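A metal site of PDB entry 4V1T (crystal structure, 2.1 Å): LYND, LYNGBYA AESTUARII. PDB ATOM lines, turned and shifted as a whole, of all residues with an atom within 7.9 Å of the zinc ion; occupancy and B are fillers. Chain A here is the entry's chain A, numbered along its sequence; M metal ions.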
ATOM      1  N   ASN A 170     -17.825  -9.106 -11.637  1.00  0.00           N
ATOM      2  CA  ASN A 170     -18.499 -10.233 -12.267  1.00  0.00           C
ATOM      3  C   ASN A 170     -17.569 -11.053 -13.163  1.00  0.00           C
ATOM      4  O   ASN A 170     -17.577 -12.293 -13.107  1.00  0.00           O
ATOM      5  CB  ASN A 170     -19.692  -9.725 -13.078  1.00  0.00           C
ATOM      6  CG  ASN A 170     -20.473 -10.850 -13.719  1.00  0.00           C
ATOM      7  OD1 ASN A 170     -20.987 -11.716 -13.028  1.00  0.00           O
ATOM      8  ND2 ASN A 170     -20.577 -10.824 -15.040  1.00  0.00           N
ATOM      9  N   LEU A 174     -16.366 -14.994 -12.561  1.00  0.00           N
ATOM     10  CA  LEU A 174     -16.548 -16.043 -13.544  1.00  0.00           C
ATOM     11  C   LEU A 174     -15.255 -16.804 -13.805  1.00  0.00           C
ATOM     12  O   LEU A 174     -15.269 -18.031 -13.885  1.00  0.00           O
ATOM     13  CB  LEU A 174     -17.098 -15.477 -14.847  1.00  0.00           C
ATOM     14  CG  LEU A 174     -18.546 -14.985 -14.762  1.00  0.00           C
ATOM     15  CD1 LEU A 174     -18.867 -14.094 -15.949  1.00  0.00           C
ATOM     16  CD2 LEU A 174     -19.501 -16.144 -14.685  1.00  0.00           C
ATOM     17  N   PHE A 196     -24.761 -15.220  -6.996  1.00  0.00           N
ATOM     18  CA  PHE A 196     -24.293 -15.693  -8.306  1.00  0.00           C
ATOM     19  C   PHE A 196     -23.419 -16.915  -8.097  1.00  0.00           C
ATOM     20  O   PHE A 196     -22.477 -16.893  -7.299  1.00  0.00           O
ATOM     21  CB  PHE A 196     -23.510 -14.602  -9.031  1.00  0.00           C
ATOM     22  CG  PHE A 196     -24.280 -13.322  -9.268  1.00  0.00           C
ATOM     23  CD1 PHE A 196     -25.113 -13.207 -10.368  1.00  0.00           C
ATOM     24  CD2 PHE A 196     -24.146 -12.242  -8.424  1.00  0.00           C
ATOM     25  CE1 PHE A 196     -25.817 -12.036 -10.608  1.00  0.00           C
ATOM     26  CE2 PHE A 196     -24.845 -11.069  -8.657  1.00  0.00           C
ATOM     27  CZ  PHE A 196     -25.681 -10.970  -9.746  1.00  0.00           C
ATOM     28  N   THR A 201     -25.918 -20.207 -12.036  1.00  0.00           N
ATOM     29  CA  THR A 201     -26.857 -19.103 -12.110  1.00  0.00           C
ATOM     30  C   THR A 201     -26.516 -18.235 -13.317  1.00  0.00           C
ATOM     31  O   THR A 201     -25.527 -18.484 -14.004  1.00  0.00           O
ATOM     32  CB  THR A 201     -26.810 -18.222 -10.845  1.00  0.00           C
ATOM     33  OG1 THR A 201     -25.552 -17.528 -10.788  1.00  0.00           O
ATOM     34  CG2 THR A 201     -26.972 -19.053  -9.580  1.00  0.00           C
ATOM     35  N   GLY A 202     -27.319 -17.207 -13.549  1.00  0.00           N
ATOM     36  CA  GLY A 202     -26.937 -16.153 -14.479  1.00  0.00           C
ATOM     37  C   GLY A 202     -25.822 -15.314 -13.868  1.00  0.00           C
ATOM     38  O   GLY A 202     -25.553 -15.409 -12.662  1.00  0.00           O
ATOM     39  N   CYS A 203     -25.141 -14.540 -14.693  1.00  0.00           N
ATOM     40  CA  CYS A 203     -24.101 -13.629 -14.219  1.00  0.00           C
ATOM     41  C   CYS A 203     -24.716 -12.244 -13.987  1.00  0.00           C
ATOM     42  O   CYS A 203     -25.899 -12.035 -14.218  1.00  0.00           O
ATOM     43  CB  CYS A 203     -22.954 -13.544 -15.241  1.00  0.00           C
ATOM     44  SG  CYS A 203     -23.328 -12.677 -16.771  1.00  0.00           S
ATOM     45  N   TRP A 204     -23.909 -11.298 -13.531  1.00  0.00           N
ATOM     46  CA  TRP A 204     -24.407  -9.934 -13.276  1.00  0.00           C
ATOM     47  C   TRP A 204     -24.844  -9.280 -14.575  1.00  0.00           C
ATOM     48  O   TRP A 204     -25.732  -8.440 -14.597  1.00  0.00           O
ATOM     49  CB  TRP A 204     -23.327  -9.085 -12.600  1.00  0.00           C
ATOM     50  CG  TRP A 204     -23.659  -7.636 -12.560  1.00  0.00           C
ATOM     51  CD1 TRP A 204     -24.388  -6.998 -11.606  1.00  0.00           C
ATOM     52  CD2 TRP A 204     -23.270  -6.642 -13.508  1.00  0.00           C
ATOM     53  NE1 TRP A 204     -24.490  -5.661 -11.905  1.00  0.00           N
ATOM     54  CE2 TRP A 204     -23.811  -5.413 -13.061  1.00  0.00           C
ATOM     55  CE3 TRP A 204     -22.517  -6.658 -14.684  1.00  0.00           C
ATOM     56  CZ2 TRP A 204     -23.635  -4.224 -13.763  1.00  0.00           C
ATOM     57  CZ3 TRP A 204     -22.337  -5.475 -15.374  1.00  0.00           C
ATOM     58  CH2 TRP A 204     -22.889  -4.274 -14.918  1.00  0.00           C
ATOM     59  N   ASP A 205     -24.225  -9.682 -15.684  1.00  0.00           N
ATOM     60  CA  ASP A 205     -24.573  -9.152 -16.999  1.00  0.00           C
ATOM     61  C   ASP A 205     -25.905  -9.718 -17.490  1.00  0.00           C
ATOM     62  O   ASP A 205     -26.645  -9.044 -18.197  1.00  0.00           O
ATOM     63  CB  ASP A 205     -23.456  -9.452 -17.997  1.00  0.00           C
ATOM     64  CG  ASP A 205     -23.374  -8.420 -19.098  1.00  0.00           C
ATOM     65  OD1 ASP A 205     -23.804  -7.262 -18.885  1.00  0.00           O
ATOM     66  OD2 ASP A 205     -22.864  -8.764 -20.186  1.00  0.00           O
ATOM     67  N   CYS A 206     -26.197 -10.968 -17.117  1.00  0.00           N
ATOM     68  CA  CYS A 206     -27.522 -11.541 -17.366  1.00  0.00           C
ATOM     69  C   CYS A 206     -28.582 -10.650 -16.725  1.00  0.00           C
ATOM     70  O   CYS A 206     -29.656 -10.408 -17.292  1.00  0.00           O
ATOM     71  CB  CYS A 206     -27.646 -12.965 -16.817  1.00  0.00           C
ATOM     72  SG  CYS A 206     -26.704 -14.237 -17.706  1.00  0.00           S
ATOM     73  N   LEU A 207     -28.272 -10.164 -15.533  1.00  0.00           N
ATOM     74  CA  LEU A 207     -29.179  -9.310 -14.766  1.00  0.00           C
ATOM     75  C   LEU A 207     -29.170  -7.889 -15.358  1.00  0.00           C
ATOM     76  O   LEU A 207     -30.227  -7.284 -15.544  1.00  0.00           O
ATOM     77  CB  LEU A 207     -28.768  -9.271 -13.300  1.00  0.00           C
ATOM     78  CG  LEU A 207     -29.552  -8.308 -12.397  1.00  0.00           C
ATOM     79  CD1 LEU A 207     -31.014  -8.735 -12.260  1.00  0.00           C
ATOM     80  CD2 LEU A 207     -28.886  -8.253 -11.035  1.00  0.00           C
ATOM     81  N   ALA A 208     -27.980  -7.383 -15.625  1.00  0.00           N
ATOM     82  CA  ALA A 208     -27.826  -6.009 -16.093  1.00  0.00           C
ATOM     83  C   ALA A 208     -28.552  -5.768 -17.419  1.00  0.00           C
ATOM     84  O   ALA A 208     -29.002  -4.664 -17.685  1.00  0.00           O
ATOM     85  CB  ALA A 208     -26.360  -5.660 -16.238  1.00  0.00           C
ATOM     86  N   LEU A 305     -33.904 -14.636 -11.541  1.00  0.00           N
ATOM     87  CA  LEU A 305     -32.918 -14.338 -12.558  1.00  0.00           C
ATOM     88  C   LEU A 305     -32.739 -15.523 -13.512  1.00  0.00           C
ATOM     89  O   LEU A 305     -32.373 -16.620 -13.087  1.00  0.00           O
ATOM     90  CB  LEU A 305     -31.574 -13.977 -11.914  1.00  0.00           C
ATOM     91  CG  LEU A 305     -30.410 -13.757 -12.903  1.00  0.00           C
ATOM     92  CD1 LEU A 305     -30.625 -12.491 -13.720  1.00  0.00           C
ATOM     93  CD2 LEU A 305     -29.086 -13.699 -12.157  1.00  0.00           C
ATOM     94  N   ILE A 306     -32.982 -15.279 -14.794  1.00  0.00           N
ATOM     95  CA  ILE A 306     -32.777 -16.297 -15.817  1.00  0.00           C
ATOM     96  C   ILE A 306     -31.374 -16.162 -16.387  1.00  0.00           C
ATOM     97  O   ILE A 306     -30.992 -15.078 -16.825  1.00  0.00           O
ATOM     98  CB  ILE A 306     -33.828 -16.181 -16.946  1.00  0.00           C
ATOM     99  CG1 ILE A 306     -35.199 -16.604 -16.447  1.00  0.00           C
ATOM    100  CG2 ILE A 306     -33.461 -17.067 -18.148  1.00  0.00           C
ATOM    101  CD1 ILE A 306     -36.138 -15.456 -16.200  1.00  0.00           C
ATOM    102  N   LYS A 307     -30.623 -17.261 -16.382  1.00  0.00           N
ATOM    103  CA  LYS A 307     -29.346 -17.329 -17.070  1.00  0.00           C
ATOM    104  C   LYS A 307     -29.591 -17.256 -18.573  1.00  0.00           C
ATOM    105  O   LYS A 307     -30.273 -18.108 -19.146  1.00  0.00           O
ATOM    106  CB  LYS A 307     -28.609 -18.626 -16.717  1.00  0.00           C
ATOM    107  CG  LYS A 307     -27.206 -18.736 -17.297  1.00  0.00           C
ATOM    108  CD  LYS A 307     -26.612 -20.128 -17.084  1.00  0.00           C
ATOM    109  CE  LYS A 307     -25.141 -20.146 -17.475  1.00  0.00           C
ATOM    110  NZ  LYS A 307     -24.598 -21.526 -17.568  1.00  0.00           N
ATOM    111  N   ARG A 308     -29.042 -16.228 -19.202  1.00  0.00           N
ATOM    112  CA  ARG A 308     -29.225 -16.010 -20.644  1.00  0.00           C
ATOM    113  C   ARG A 308     -28.193 -16.811 -21.399  1.00  0.00           C
ATOM    114  O   ARG A 308     -26.996 -16.533 -21.321  1.00  0.00           O
ATOM    115  CB  ARG A 308     -29.113 -14.523 -20.980  1.00  0.00           C
ATOM    116  CG  ARG A 308     -29.973 -13.631 -20.119  1.00  0.00           C
ATOM    117  CD  ARG A 308     -29.824 -12.168 -20.501  1.00  0.00           C
ATOM    118  NE  ARG A 308     -30.404 -11.879 -21.817  1.00  0.00           N
ATOM    119  CZ  ARG A 308     -29.740 -11.362 -22.852  1.00  0.00           C
ATOM    120  NH1 ARG A 308     -28.451 -11.037 -22.747  1.00  0.00           N
ATOM    121  NH2 ARG A 308     -30.368 -11.133 -23.992  1.00  0.00           N
ATOM    122  N   SER A 309     -28.639 -17.817 -22.147  1.00  0.00           N
ATOM    123  CA  SER A 309     -27.708 -18.653 -22.913  1.00  0.00           C
ATOM    124  C   SER A 309     -26.928 -17.843 -23.958  1.00  0.00           C
ATOM    125  O   SER A 309     -25.853 -18.271 -24.386  1.00  0.00           O
ATOM    126  CB  SER A 309     -28.451 -19.802 -23.601  1.00  0.00           C
ATOM    127  OG  SER A 309     -29.386 -19.309 -24.546  1.00  0.00           O
ATOM    128  N   GLN A 310     -27.478 -16.703 -24.391  1.00  0.00           N
ATOM    129  CA  GLN A 310     -26.803 -15.855 -25.368  1.00  0.00           C
ATOM    130  C   GLN A 310     -26.065 -14.695 -24.722  1.00  0.00           C
ATOM    131  O   GLN A 310     -25.671 -13.737 -25.399  1.00  0.00           O
ATOM    132  CB  GLN A 310     -27.790 -15.315 -26.429  1.00  0.00           C
ATOM    133  CG  GLN A 310     -28.703 -14.175 -25.994  1.00  0.00           C
ATOM    134  CD  GLN A 310     -29.890 -14.655 -25.180  1.00  0.00           C
ATOM    135  OE1 GLN A 310     -29.760 -15.533 -24.323  1.00  0.00           O
ATOM    136  NE2 GLN A 310     -31.056 -14.077 -25.445  1.00  0.00           N
ATOM    137  N   CYS A 311     -25.856 -14.788 -23.400  1.00  0.00           N
ATOM    138  CA  CYS A 311     -25.131 -13.747 -22.662  1.00  0.00           C
ATOM    139  C   CYS A 311     -23.733 -13.591 -23.237  1.00  0.00           C
ATOM    140  O   CYS A 311     -22.999 -14.571 -23.355  1.00  0.00           O
ATOM    141  CB  CYS A 311     -25.031 -14.089 -21.178  1.00  0.00           C
ATOM    142  SG  CYS A 311     -24.065 -12.960 -20.143  1.00  0.00           S
ATOM    143  N   PRO A 312     -23.352 -12.360 -23.592  1.00  0.00           N
ATOM    144  CA  PRO A 312     -21.999 -12.164 -24.176  1.00  0.00           C
ATOM    145  C   PRO A 312     -20.878 -12.340 -23.159  1.00  0.00           C
ATOM    146  O   PRO A 312     -19.714 -12.469 -23.537  1.00  0.00           O
ATOM    147  CB  PRO A 312     -22.045 -10.709 -24.671  1.00  0.00           C
ATOM    148  CG  PRO A 312     -23.081 -10.063 -23.841  1.00  0.00           C
ATOM    149  CD  PRO A 312     -24.120 -11.111 -23.571  1.00  0.00           C
ATOM    150  N   THR A 313     -21.216 -12.357 -21.867  1.00  0.00           N
ATOM    151  CA  THR A 313     -20.211 -12.470 -20.825  1.00  0.00           C
ATOM    152  C   THR A 313     -20.062 -13.898 -20.331  1.00  0.00           C
ATOM    153  O   THR A 313     -18.962 -14.363 -20.134  1.00  0.00           O
ATOM    154  CB  THR A 313     -20.555 -11.564 -19.623  1.00  0.00           C
ATOM    155  OG1 THR A 313     -20.681 -10.209 -20.075  1.00  0.00           O
ATOM    156  CG2 THR A 313     -19.481 -11.626 -18.552  1.00  0.00           C
ATOM    157  N   CYS A 314     -21.180 -14.591 -20.091  1.00  0.00           N
ATOM    158  CA  CYS A 314     -21.130 -15.937 -19.514  1.00  0.00           C
ATOM    159  C   CYS A 314     -21.707 -17.017 -20.423  1.00  0.00           C
ATOM    160  O   CYS A 314     -21.777 -18.173 -20.040  1.00  0.00           O
ATOM    161  CB  CYS A 314     -21.870 -15.935 -18.164  1.00  0.00           C
ATOM    162  SG  CYS A 314     -23.676 -16.039 -18.252  1.00  0.00           S
ATOM    163  N   GLY A 315     -22.130 -16.644 -21.631  1.00  0.00           N
ATOM    164  CA  GLY A 315     -22.752 -17.582 -22.555  1.00  0.00           C
ATOM    165  C   GLY A 315     -22.183 -17.506 -23.966  1.00  0.00           C
ATOM    166  O   GLY A 315     -21.001 -17.274 -24.142  1.00  0.00           O
HETATM  167 ZN    ZN M   1     -24.423 -13.903 -18.081  1.00  0.00          ZN
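The backbone NH (N) of Asp 205 lies close to the side-chain sulfur (SG) of Cys 203 (3.3 Å).
The side-chain amide nitrogen (ND2) of Asn 170 sits close to the side-chain sulfur (SG) of Cys 203 (3.7 Å).
N of Thr 313 lies close to SG of Cys 311 (3.4 Å).
The side-chain sulfur (SG) of Cys 206 lies close to the backbone NH (N) of Arg 308, at 3.4 Å.
Of the 22 residues printed, 4 come within 4 Å of the zinc ion.
The zinc ion is bound by SG of Cys 203 (2.1 Å), SG of Cys 314 (2.3 Å), SG of Cys 311 (2.3 Å) and SG of Cys 206 (2.3 Å).
The zinc ion has four donor atoms within binding distance.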
